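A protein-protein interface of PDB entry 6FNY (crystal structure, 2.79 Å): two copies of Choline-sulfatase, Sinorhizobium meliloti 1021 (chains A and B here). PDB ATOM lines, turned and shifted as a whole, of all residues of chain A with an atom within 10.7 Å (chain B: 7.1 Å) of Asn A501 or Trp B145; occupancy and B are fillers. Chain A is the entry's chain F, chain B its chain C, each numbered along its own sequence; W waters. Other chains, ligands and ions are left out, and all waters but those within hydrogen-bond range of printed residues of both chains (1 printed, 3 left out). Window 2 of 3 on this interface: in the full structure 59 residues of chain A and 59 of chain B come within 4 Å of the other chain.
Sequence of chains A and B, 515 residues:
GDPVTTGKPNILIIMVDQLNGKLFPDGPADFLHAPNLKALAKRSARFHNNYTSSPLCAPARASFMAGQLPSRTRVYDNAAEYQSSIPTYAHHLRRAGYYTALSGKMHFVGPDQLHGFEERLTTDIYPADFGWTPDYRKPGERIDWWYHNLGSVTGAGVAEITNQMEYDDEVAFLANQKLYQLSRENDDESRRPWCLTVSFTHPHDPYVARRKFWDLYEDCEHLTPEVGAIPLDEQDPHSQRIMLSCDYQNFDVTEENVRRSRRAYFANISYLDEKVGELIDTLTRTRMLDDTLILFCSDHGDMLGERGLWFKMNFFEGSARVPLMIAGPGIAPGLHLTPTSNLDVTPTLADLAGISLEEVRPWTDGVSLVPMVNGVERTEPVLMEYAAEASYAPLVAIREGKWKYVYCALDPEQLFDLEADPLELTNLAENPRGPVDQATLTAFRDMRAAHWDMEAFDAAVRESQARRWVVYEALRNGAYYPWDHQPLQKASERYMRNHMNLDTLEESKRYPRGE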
ATOM      1  N   TYR A 495      15.704 -20.996  10.679  1.00  0.00           N
ATOM      2  CA  TYR A 495      17.019 -21.645  10.770  1.00  0.00           C
ATOM      3  C   TYR A 495      17.232 -22.466   9.498  1.00  0.00           C
ATOM      4  O   TYR A 495      16.948 -21.962   8.401  1.00  0.00           O
ATOM      5  CB  TYR A 495      17.097 -22.414  12.083  1.00  0.00           C
ATOM      6  CG  TYR A 495      16.785 -21.557  13.289  1.00  0.00           C
ATOM      7  CD1 TYR A 495      17.577 -20.460  13.608  1.00  0.00           C
ATOM      8  CD2 TYR A 495      15.694 -21.835  14.102  1.00  0.00           C
ATOM      9  CE1 TYR A 495      17.295 -19.668  14.706  1.00  0.00           C
ATOM     10  CE2 TYR A 495      15.404 -21.049  15.203  1.00  0.00           C
ATOM     11  CZ  TYR A 495      16.208 -19.968  15.500  1.00  0.00           C
ATOM     12  OH  TYR A 495      15.924 -19.183  16.596  1.00  0.00           O
ATOM     13  N   MET A 496      17.717 -23.703   9.585  1.00  0.00           N
ATOM     14  CA  MET A 496      18.087 -24.488   8.414  1.00  0.00           C
ATOM     15  C   MET A 496      17.034 -25.558   8.159  1.00  0.00           C
ATOM     16  O   MET A 496      16.796 -26.419   9.013  1.00  0.00           O
ATOM     17  CB  MET A 496      19.467 -25.122   8.598  1.00  0.00           C
ATOM     18  CG  MET A 496      19.930 -25.959   7.412  1.00  0.00           C
ATOM     19  SD  MET A 496      19.729 -25.119   5.826  1.00  0.00           S
ATOM     20  CE  MET A 496      20.177 -26.421   4.680  1.00  0.00           C
ATOM     21  N   ARG A 497      16.407 -25.498   6.986  1.00  0.00           N
ATOM     22  CA  ARG A 497      15.487 -26.523   6.517  1.00  0.00           C
ATOM     23  C   ARG A 497      15.899 -26.943   5.113  1.00  0.00           C
ATOM     24  O   ARG A 497      16.425 -26.140   4.338  1.00  0.00           O
ATOM     25  CB  ARG A 497      14.035 -26.029   6.529  1.00  0.00           C
ATOM     26  CG  ARG A 497      13.607 -25.387   7.846  1.00  0.00           C
ATOM     27  CD  ARG A 497      13.464 -26.430   8.940  1.00  0.00           C
ATOM     28  NE  ARG A 497      13.133 -25.847  10.238  1.00  0.00           N
ATOM     29  CZ  ARG A 497      13.915 -25.921  11.313  1.00  0.00           C
ATOM     30  NH1 ARG A 497      15.082 -26.551  11.247  1.00  0.00           N
ATOM     31  NH2 ARG A 497      13.534 -25.366  12.456  1.00  0.00           N
ATOM     32  N   ASN A 498      15.650 -28.211   4.786  1.00  0.00           N
ATOM     33  CA  ASN A 498      16.233 -28.829   3.600  1.00  0.00           C
ATOM     34  C   ASN A 498      15.537 -28.442   2.297  1.00  0.00           C
ATOM     35  O   ASN A 498      15.627 -29.196   1.319  1.00  0.00           O
ATOM     36  CB  ASN A 498      16.249 -30.349   3.759  1.00  0.00           C
ATOM     37  CG  ASN A 498      17.510 -30.842   4.430  1.00  0.00           C
ATOM     38  OD1 ASN A 498      18.558 -30.201   4.345  1.00  0.00           O
ATOM     39  ND2 ASN A 498      17.419 -31.981   5.108  1.00  0.00           N
ATOM     40  N   HIS A 499      14.853 -27.301   2.248  1.00  0.00           N
ATOM     41  CA  HIS A 499      14.420 -26.711   0.988  1.00  0.00           C
ATOM     42  C   HIS A 499      15.243 -25.481   0.632  1.00  0.00           C
ATOM     43  O   HIS A 499      14.895 -24.761  -0.311  1.00  0.00           O
ATOM     44  CB  HIS A 499      12.927 -26.363   1.035  1.00  0.00           C
ATOM     45  CG  HIS A 499      12.550 -25.443   2.154  1.00  0.00           C
ATOM     46  ND1 HIS A 499      12.069 -25.899   3.363  1.00  0.00           N
ATOM     47  CD2 HIS A 499      12.577 -24.092   2.246  1.00  0.00           C
ATOM     48  CE1 HIS A 499      11.817 -24.869   4.152  1.00  0.00           C
ATOM     49  NE2 HIS A 499      12.117 -23.762   3.498  1.00  0.00           N
ATOM     50  N   MET A 500      16.325 -25.228   1.362  1.00  0.00           N
ATOM     51  CA  MET A 500      17.221 -24.104   1.132  1.00  0.00           C
ATOM     52  C   MET A 500      18.620 -24.630   0.816  1.00  0.00           C
ATOM     53  O   MET A 500      18.813 -25.812   0.515  1.00  0.00           O
ATOM     54  CB  MET A 500      17.248 -23.178   2.350  1.00  0.00           C
ATOM     55  CG  MET A 500      15.927 -23.042   3.090  1.00  0.00           C
ATOM     56  SD  MET A 500      16.048 -21.848   4.439  1.00  0.00           S
ATOM     57  CE  MET A 500      15.246 -22.726   5.773  1.00  0.00           C
ATOM     58  N   ASN A 501      19.601 -23.733   0.894  1.00  0.00           N
ATOM     59  CA  ASN A 501      21.013 -24.080   0.788  1.00  0.00           C
ATOM     60  C   ASN A 501      21.730 -23.511   2.002  1.00  0.00           C
ATOM     61  O   ASN A 501      21.553 -22.335   2.332  1.00  0.00           O
ATOM     62  CB  ASN A 501      21.630 -23.539  -0.507  1.00  0.00           C
ATOM     63  CG  ASN A 501      23.055 -24.020  -0.724  1.00  0.00           C
ATOM     64  OD1 ASN A 501      23.972 -23.631   0.001  1.00  0.00           O
ATOM     65  ND2 ASN A 501      23.248 -24.867  -1.728  1.00  0.00           N
ATOM     66  N   LEU A 502      22.537 -24.347   2.661  1.00  0.00           N
ATOM     67  CA  LEU A 502      23.161 -23.948   3.920  1.00  0.00           C
ATOM     68  C   LEU A 502      24.064 -22.733   3.735  1.00  0.00           C
ATOM     69  O   LEU A 502      24.009 -21.779   4.519  1.00  0.00           O
ATOM     70  CB  LEU A 502      23.947 -25.119   4.511  1.00  0.00           C
ATOM     71  CG  LEU A 502      24.559 -24.883   5.894  1.00  0.00           C
ATOM     72  CD1 LEU A 502      23.547 -25.182   6.996  1.00  0.00           C
ATOM     73  CD2 LEU A 502      25.824 -25.712   6.079  1.00  0.00           C
ATOM     74  N   ASP A 503      24.904 -22.750   2.698  1.00  0.00           N
ATOM     75  CA  ASP A 503      25.840 -21.649   2.495  1.00  0.00           C
ATOM     76  C   ASP A 503      25.130 -20.373   2.058  1.00  0.00           C
ATOM     77  O   ASP A 503      25.565 -19.273   2.413  1.00  0.00           O
ATOM     78  CB  ASP A 503      26.906 -22.049   1.475  1.00  0.00           C
ATOM     79  CG  ASP A 503      27.791 -23.175   1.974  1.00  0.00           C
ATOM     80  OD1 ASP A 503      27.868 -23.369   3.206  1.00  0.00           O
ATOM     81  OD2 ASP A 503      28.410 -23.862   1.134  1.00  0.00           O
ATOM     82  N   THR A 504      24.044 -20.496   1.292  1.00  0.00           N
ATOM     83  CA  THR A 504      23.259 -19.319   0.935  1.00  0.00           C
ATOM     84  C   THR A 504      22.502 -18.780   2.143  1.00  0.00           C
ATOM     85  O   THR A 504      22.349 -17.562   2.297  1.00  0.00           O
ATOM     86  CB  THR A 504      22.290 -19.657  -0.200  1.00  0.00           C
ATOM     87  OG1 THR A 504      23.022 -20.198  -1.306  1.00  0.00           O
ATOM     88  CG2 THR A 504      21.539 -18.413  -0.659  1.00  0.00           C
ATOM     89  N   LEU A 505      22.034 -19.673   3.018  1.00  0.00           N
ATOM     90  CA  LEU A 505      21.279 -19.245   4.191  1.00  0.00           C
ATOM     91  C   LEU A 505      22.173 -18.542   5.207  1.00  0.00           C
ATOM     92  O   LEU A 505      21.774 -17.528   5.794  1.00  0.00           O
ATOM     93  CB  LEU A 505      20.588 -20.449   4.828  1.00  0.00           C
ATOM     94  CG  LEU A 505      20.030 -20.249   6.238  1.00  0.00           C
ATOM     95  CD1 LEU A 505      18.640 -19.633   6.182  1.00  0.00           C
ATOM     96  CD2 LEU A 505      20.015 -21.566   6.995  1.00  0.00           C
ATOM     97  N   GLU A 506      23.384 -19.062   5.428  1.00  0.00           N
ATOM     98  CA  GLU A 506      24.257 -18.491   6.449  1.00  0.00           C
ATOM     99  C   GLU A 506      24.631 -17.050   6.122  1.00  0.00           C
ATOM    100  O   GLU A 506      24.712 -16.204   7.021  1.00  0.00           O
ATOM    101  CB  GLU A 506      25.512 -19.348   6.608  1.00  0.00           C
ATOM    102  CG  GLU A 506      25.274 -20.691   7.289  1.00  0.00           C
ATOM    103  CD  GLU A 506      25.041 -20.570   8.787  1.00  0.00           C
ATOM    104  OE1 GLU A 506      24.671 -21.586   9.412  1.00  0.00           O
ATOM    105  OE2 GLU A 506      25.227 -19.466   9.341  1.00  0.00           O
ATOM    106  N   GLU A 507      24.860 -16.747   4.843  1.00  0.00           N
ATOM    107  CA  GLU A 507      25.197 -15.378   4.466  1.00  0.00           C
ATOM    108  C   GLU A 507      23.993 -14.454   4.607  1.00  0.00           C
ATOM    109  O   GLU A 507      24.140 -13.284   4.982  1.00  0.00           O
ATOM    110  CB  GLU A 507      25.743 -15.349   3.036  1.00  0.00           C
ATOM    111  CG  GLU A 507      25.930 -13.952   2.456  1.00  0.00           C
ATOM    112  CD  GLU A 507      27.292 -13.358   2.768  1.00  0.00           C
ATOM    113  OE1 GLU A 507      27.976 -13.864   3.683  1.00  0.00           O
ATOM    114  OE2 GLU A 507      27.675 -12.375   2.099  1.00  0.00           O
ATOM    115  N   SER A 508      22.792 -14.963   4.326  1.00  0.00           N
ATOM    116  CA  SER A 508      21.604 -14.118   4.391  1.00  0.00           C
ATOM    117  C   SER A 508      21.203 -13.820   5.831  1.00  0.00           C
ATOM    118  O   SER A 508      20.634 -12.756   6.105  1.00  0.00           O
ATOM    119  CB  SER A 508      20.447 -14.775   3.637  1.00  0.00           C
ATOM    120  OG  SER A 508      19.847 -15.803   4.408  1.00  0.00           O
ATOM    121  N   LYS A 509      21.487 -14.732   6.758  1.00  0.00           N
ATOM    122  CA  LYS A 509      21.176 -14.527   8.167  1.00  0.00           C
ATOM    123  C   LYS A 509      22.278 -13.785   8.909  1.00  0.00           C
ATOM    124  O   LYS A 509      22.107 -13.464  10.090  1.00  0.00           O
ATOM    125  CB  LYS A 509      20.911 -15.871   8.854  1.00  0.00           C
ATOM    126  CG  LYS A 509      19.746 -16.651   8.263  1.00  0.00           C
ATOM    127  CD  LYS A 509      18.459 -15.844   8.307  1.00  0.00           C
ATOM    128  CE  LYS A 509      17.332 -16.565   7.586  1.00  0.00           C
ATOM    129  NZ  LYS A 509      16.080 -15.758   7.549  1.00  0.00           N
ATOM    130  N   PRO B 127      17.841 -29.369  10.088  1.00  0.00           N
ATOM    131  CA  PRO B 127      16.646 -30.065   9.596  1.00  0.00           C
ATOM    132  C   PRO B 127      16.387 -31.368  10.338  1.00  0.00           C
ATOM    133  O   PRO B 127      17.259 -31.924  11.009  1.00  0.00           O
ATOM    134  CB  PRO B 127      16.968 -30.326   8.121  1.00  0.00           C
ATOM    135  CG  PRO B 127      17.986 -29.298   7.771  1.00  0.00           C
ATOM    136  CD  PRO B 127      18.806 -29.106   9.007  1.00  0.00           C
ATOM    137  N   ASP B 129      14.596 -34.027   8.614  1.00  0.00           N
ATOM    138  CA  ASP B 129      14.197 -34.978   7.587  1.00  0.00           C
ATOM    139  C   ASP B 129      15.399 -35.817   7.150  1.00  0.00           C
ATOM    140  O   ASP B 129      16.494 -35.717   7.714  1.00  0.00           O
ATOM    141  CB  ASP B 129      13.561 -34.239   6.404  1.00  0.00           C
ATOM    142  CG  ASP B 129      14.396 -33.061   5.927  1.00  0.00           C
ATOM    143  OD1 ASP B 129      15.620 -33.052   6.174  1.00  0.00           O
ATOM    144  OD2 ASP B 129      13.825 -32.140   5.305  1.00  0.00           O
ATOM    145  N   PHE B 130      15.190 -36.647   6.124  1.00  0.00           N
ATOM    146  CA  PHE B 130      16.227 -37.528   5.600  1.00  0.00           C
ATOM    147  C   PHE B 130      17.041 -36.882   4.485  1.00  0.00           C
ATOM    148  O   PHE B 130      17.550 -37.589   3.605  1.00  0.00           O
ATOM    149  CB  PHE B 130      15.607 -38.835   5.105  1.00  0.00           C
ATOM    150  CG  PHE B 130      14.716 -39.510   6.109  1.00  0.00           C
ATOM    151  CD1 PHE B 130      15.035 -39.508   7.458  1.00  0.00           C
ATOM    152  CD2 PHE B 130      13.557 -40.151   5.701  1.00  0.00           C
ATOM    153  CE1 PHE B 130      14.212 -40.131   8.380  1.00  0.00           C
ATOM    154  CE2 PHE B 130      12.730 -40.776   6.618  1.00  0.00           C
ATOM    155  CZ  PHE B 130      13.058 -40.766   7.958  1.00  0.00           C
ATOM    156  N   GLY B 131      17.183 -35.556   4.499  1.00  0.00           N
ATOM    157  CA  GLY B 131      17.866 -34.891   3.402  1.00  0.00           C
ATOM    158  C   GLY B 131      19.361 -35.146   3.388  1.00  0.00           C
ATOM    159  O   GLY B 131      19.942 -35.418   2.333  1.00  0.00           O
ATOM    160  N   TRP B 132      20.004 -35.066   4.552  1.00  0.00           N
ATOM    161  CA  TRP B 132      21.455 -35.189   4.633  1.00  0.00           C
ATOM    162  C   TRP B 132      21.890 -36.647   4.731  1.00  0.00           C
ATOM    163  O   TRP B 132      22.688 -37.003   5.604  1.00  0.00           O
ATOM    164  CB  TRP B 132      21.990 -34.405   5.834  1.00  0.00           C
ATOM    165  CG  TRP B 132      21.707 -32.940   5.794  1.00  0.00           C
ATOM    166  CD1 TRP B 132      21.064 -32.256   4.809  1.00  0.00           C
ATOM    167  CD2 TRP B 132      22.061 -31.972   6.792  1.00  0.00           C
ATOM    168  NE1 TRP B 132      20.994 -30.922   5.126  1.00  0.00           N
ATOM    169  CE2 TRP B 132      21.599 -30.721   6.338  1.00  0.00           C
ATOM    170  CE3 TRP B 132      22.724 -32.041   8.022  1.00  0.00           C
ATOM    171  CZ2 TRP B 132      21.776 -29.548   7.071  1.00  0.00           C
ATOM    172  CZ3 TRP B 132      22.901 -30.873   8.750  1.00  0.00           C
ATOM    173  CH2 TRP B 132      22.428 -29.644   8.270  1.00  0.00           C
ATOM    174  N   THR B 133      21.378 -37.500   3.840  1.00  0.00           N
ATOM    175  CA  THR B 133      21.658 -38.928   3.899  1.00  0.00           C
ATOM    176  C   THR B 133      22.811 -39.270   2.971  1.00  0.00           C
ATOM    177  O   THR B 133      22.706 -39.033   1.757  1.00  0.00           O
ATOM    178  CB  THR B 133      20.421 -39.734   3.520  1.00  0.00           C
ATOM    179  OG1 THR B 133      19.438 -39.614   4.556  1.00  0.00           O
ATOM    180  CG2 THR B 133      20.771 -41.203   3.332  1.00  0.00           C
ATOM    181  N   ARG B 142      30.160 -36.098  -3.683  1.00  0.00           N
ATOM    182  CA  ARG B 142      30.042 -34.984  -2.756  1.00  0.00           C
ATOM    183  C   ARG B 142      28.763 -34.227  -3.075  1.00  0.00           C
ATOM    184  O   ARG B 142      28.420 -34.040  -4.246  1.00  0.00           O
ATOM    185  CB  ARG B 142      31.257 -34.048  -2.843  1.00  0.00           C
ATOM    186  CG  ARG B 142      31.132 -32.798  -1.990  1.00  0.00           C
ATOM    187  CD  ARG B 142      32.322 -31.872  -2.162  1.00  0.00           C
ATOM    188  NE  ARG B 142      32.256 -30.751  -1.230  1.00  0.00           N
ATOM    189  CZ  ARG B 142      31.525 -29.658  -1.427  1.00  0.00           C
ATOM    190  NH1 ARG B 142      30.800 -29.533  -2.530  1.00  0.00           N
ATOM    191  NH2 ARG B 142      31.523 -28.687  -0.525  1.00  0.00           N
ATOM    192  N   ILE B 143      28.054 -33.805  -2.032  1.00  0.00           N
ATOM    193  CA  ILE B 143      26.773 -33.120  -2.167  1.00  0.00           C
ATOM    194  C   ILE B 143      26.953 -31.702  -1.641  1.00  0.00           C
ATOM    195  O   ILE B 143      27.029 -31.488  -0.426  1.00  0.00           O
ATOM    196  CB  ILE B 143      25.654 -33.858  -1.424  1.00  0.00           C
ATOM    197  CG1 ILE B 143      25.694 -35.348  -1.769  1.00  0.00           C
ATOM    198  CG2 ILE B 143      24.310 -33.272  -1.781  1.00  0.00           C
ATOM    199  CD1 ILE B 143      24.633 -36.173  -1.081  1.00  0.00           C
ATOM    200  N   ASP B 144      26.994 -30.729  -2.554  1.00  0.00           N
ATOM    201  CA  ASP B 144      27.464 -29.394  -2.195  1.00  0.00           C
ATOM    202  C   ASP B 144      26.502 -28.658  -1.268  1.00  0.00           C
ATOM    203  O   ASP B 144      26.943 -27.842  -0.451  1.00  0.00           O
ATOM    204  CB  ASP B 144      27.709 -28.571  -3.460  1.00  0.00           C
ATOM    205  CG  ASP B 144      28.523 -27.318  -3.193  1.00  0.00           C
ATOM    206  OD1 ASP B 144      29.619 -27.435  -2.607  1.00  0.00           O
ATOM    207  OD2 ASP B 144      28.069 -26.216  -3.572  1.00  0.00           O
ATOM    208  N   TRP B 145      25.199 -28.920  -1.366  1.00  0.00           N
ATOM    209  CA  TRP B 145      24.241 -28.056  -0.685  1.00  0.00           C
ATOM    210  C   TRP B 145      24.096 -28.348   0.806  1.00  0.00           C
ATOM    211  O   TRP B 145      23.294 -27.678   1.466  1.00  0.00           O
ATOM    212  CB  TRP B 145      22.868 -28.129  -1.369  1.00  0.00           C
ATOM    213  CG  TRP B 145      22.263 -29.498  -1.473  1.00  0.00           C
ATOM    214  CD1 TRP B 145      22.428 -30.390  -2.491  1.00  0.00           C
ATOM    215  CD2 TRP B 145      21.368 -30.116  -0.538  1.00  0.00           C
ATOM    216  NE1 TRP B 145      21.701 -31.529  -2.245  1.00  0.00           N
ATOM    217  CE2 TRP B 145      21.045 -31.388  -1.051  1.00  0.00           C
ATOM    218  CE3 TRP B 145      20.818 -29.720   0.685  1.00  0.00           C
ATOM    219  CZ2 TRP B 145      20.194 -32.269  -0.383  1.00  0.00           C
ATOM    220  CZ3 TRP B 145      19.973 -30.596   1.347  1.00  0.00           C
ATOM    221  CH2 TRP B 145      19.670 -31.855   0.811  1.00  0.00           C
ATOM    222  N   TRP B 146      24.845 -29.301   1.361  1.00  0.00           N
ATOM    223  CA  TRP B 146      24.811 -29.500   2.808  1.00  0.00           C
ATOM    224  C   TRP B 146      26.115 -30.074   3.351  1.00  0.00           C
ATOM    225  O   TRP B 146      26.288 -30.175   4.571  1.00  0.00           O
ATOM    226  CB  TRP B 146      23.629 -30.393   3.204  1.00  0.00           C
ATOM    227  CG  TRP B 146      23.696 -31.811   2.713  1.00  0.00           C
ATOM    228  CD1 TRP B 146      23.151 -32.305   1.564  1.00  0.00           C
ATOM    229  CD2 TRP B 146      24.319 -32.922   3.370  1.00  0.00           C
ATOM    230  NE1 TRP B 146      23.404 -33.651   1.458  1.00  0.00           N
ATOM    231  CE2 TRP B 146      24.121 -34.055   2.554  1.00  0.00           C
ATOM    232  CE3 TRP B 146      25.031 -33.069   4.565  1.00  0.00           C
ATOM    233  CZ2 TRP B 146      24.607 -35.316   2.894  1.00  0.00           C
ATOM    234  CZ3 TRP B 146      25.512 -34.323   4.901  1.00  0.00           C
ATOM    235  CH2 TRP B 146      25.298 -35.429   4.068  1.00  0.00           C
ATOM    236  N   TYR B 147      27.041 -30.444   2.469  1.00  0.00           N
ATOM    237  CA  TYR B 147      28.347 -30.900   2.919  1.00  0.00           C
ATOM    238  C   TYR B 147      29.137 -29.746   3.528  1.00  0.00           C
ATOM    239  O   TYR B 147      28.885 -28.568   3.255  1.00  0.00           O
ATOM    240  CB  TYR B 147      29.147 -31.500   1.764  1.00  0.00           C
ATOM    241  CG  TYR B 147      29.054 -33.003   1.645  1.00  0.00           C
ATOM    242  CD1 TYR B 147      27.826 -33.650   1.714  1.00  0.00           C
ATOM    243  CD2 TYR B 147      30.193 -33.775   1.456  1.00  0.00           C
ATOM    244  CE1 TYR B 147      27.737 -35.024   1.600  1.00  0.00           C
ATOM    245  CE2 TYR B 147      30.113 -35.151   1.341  1.00  0.00           C
ATOM    246  CZ  TYR B 147      28.881 -35.769   1.415  1.00  0.00           C
ATOM    247  OH  TYR B 147      28.794 -37.138   1.303  1.00  0.00           O
ATOM    248  N   ASN B 149      32.371 -27.391   3.775  1.00  0.00           N
ATOM    249  CA  ASN B 149      33.366 -26.881   2.843  1.00  0.00           C
ATOM    250  C   ASN B 149      34.167 -25.790   3.536  1.00  0.00           C
ATOM    251  O   ASN B 149      33.707 -25.170   4.500  1.00  0.00           O
ATOM    252  CB  ASN B 149      32.731 -26.362   1.542  1.00  0.00           C
ATOM    253  CG  ASN B 149      31.740 -25.238   1.774  1.00  0.00           C
ATOM    254  OD1 ASN B 149      32.122 -24.110   2.089  1.00  0.00           O
ATOM    255  ND2 ASN B 149      30.457 -25.538   1.603  1.00  0.00           N
ATOM    256  N   TRP B 469      16.533 -43.215   1.021  1.00  0.00           N
ATOM    257  CA  TRP B 469      16.539 -42.550  -0.278  1.00  0.00           C
ATOM    258  C   TRP B 469      15.248 -42.793  -1.045  1.00  0.00           C
ATOM    259  O   TRP B 469      14.803 -41.920  -1.796  1.00  0.00           O
ATOM    260  CB  TRP B 469      17.749 -42.999  -1.095  1.00  0.00           C
ATOM    261  CG  TRP B 469      18.951 -42.139  -0.861  1.00  0.00           C
ATOM    262  CD1 TRP B 469      20.187 -42.550  -0.452  1.00  0.00           C
ATOM    263  CD2 TRP B 469      19.031 -40.713  -1.010  1.00  0.00           C
ATOM    264  NE1 TRP B 469      21.032 -41.472  -0.341  1.00  0.00           N
ATOM    265  CE2 TRP B 469      20.347 -40.333  -0.678  1.00  0.00           C
ATOM    266  CE3 TRP B 469      18.118 -39.723  -1.394  1.00  0.00           C
ATOM    267  CZ2 TRP B 469      20.773 -39.005  -0.718  1.00  0.00           C
ATOM    268  CZ3 TRP B 469      18.544 -38.405  -1.433  1.00  0.00           C
ATOM    269  CH2 TRP B 469      19.860 -38.058  -1.097  1.00  0.00           C
ATOM    270  N   TYR B 472      12.685 -40.525   1.352  1.00  0.00           N
ATOM    271  CA  TYR B 472      12.864 -39.087   1.174  1.00  0.00           C
ATOM    272  C   TYR B 472      12.533 -38.657  -0.247  1.00  0.00           C
ATOM    273  O   TYR B 472      12.169 -37.498  -0.478  1.00  0.00           O
ATOM    274  CB  TYR B 472      14.293 -38.677   1.534  1.00  0.00           C
ATOM    275  CG  TYR B 472      14.496 -37.179   1.602  1.00  0.00           C
ATOM    276  CD1 TYR B 472      13.922 -36.427   2.619  1.00  0.00           C
ATOM    277  CD2 TYR B 472      15.257 -36.516   0.647  1.00  0.00           C
ATOM    278  CE1 TYR B 472      14.101 -35.056   2.685  1.00  0.00           C
ATOM    279  CE2 TYR B 472      15.443 -35.147   0.706  1.00  0.00           C
ATOM    280  CZ  TYR B 472      14.861 -34.422   1.726  1.00  0.00           C
ATOM    281  OH  TYR B 472      15.040 -33.060   1.790  1.00  0.00           O
HETATM  282  O   HOH W   1      27.123 -26.459   3.181  1.00  0.00           O
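The indole nitrogen (NE1) of Trp B132 lies within hydrogen-bond range of the side-chain amide oxygen (OD1) of Asn A498, 2.7 Å away.
ND2 of Asn B149 is in hydrogen-bond range of OD2 of Asp A503 (2.7 Å).
O of Met A496 sits close to N of Pro B127 (3.3 Å).
The side-chain amide nitrogen (ND2) of Asn A498 lies close to the side-chain carboxylate (OD1) of Asp B129.
The side-chain carboxylate (OD1) of Asp B129 sits close to the backbone NH (N) of Gly B131 (3.4 Å).
The side-chain amide oxygen (OD1) of Asn A501 sits at hydrogen-bond distance from the backbone NH (N) of Asp A503, at 3.0 Å.
OD1 of Asn A501 sits at hydrogen-bond distance from N of Thr A504, at 3.4 Å.
Among the printed residues, merely in contact across the chains: Asn A501 with Trp B145 (3.3 Å), Asn A498 with Trp B145 (3.3 Å), Asn A498 with Gly B131 (3.4 Å), Asn A498 with Pro B127 (3.5 Å), Asn A498 with Tyr B472 (3.6 Å), Leu A502 with Trp B145 (3.6 Å) and Arg A497 with Pro B127 (3.9 Å).
Of chain A, only Asn A498 comes within 4 Å of Gly B131.
No residue of chain A comes within 4 Å of Ile B143.
No residue of chain A comes within 4 Å of Asp B144.
Printed residues of chain A within 4 Å of Tyr B472: Asn A498.
Printed residues of chain A within 4 Å of Asp B129: Asn A498.
Tyr A495 touches none of the printed residues of chain B.
Ser A508 touches none of the printed residues of chain B.
The nearest residue of chain B that does not touch Asn A501 is Asp B144 (4.9 Å).
The nearest printed residue of chain A that does not touch Asn B149 is Leu A502 (6.4 Å).
Of the 15 printed residues of chain A, 6 touch a printed residue of chain B.
Printed residues of chain A that touch a printed residue of chain B: Met A496, Arg A497, Asn A498, Asn A501, Leu A502 and Asp A503.
Hydrophobic or aromatic side chains of chain A within 4 Å of the printed part of chain B: Met A496.
Among the printed residues, 11 pairs touch across the chains.
Among the printed residues, no Asp or Glu carboxylate lies within 4 Å of a Lys or Arg side-chain nitrogen of the other chain.
No position is printed for both chains.
Water W1 lies within hydrogen-bond range of O of Tyr B147 (2.7 Å) and OD1 of Asp A503 (3.2 Å).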
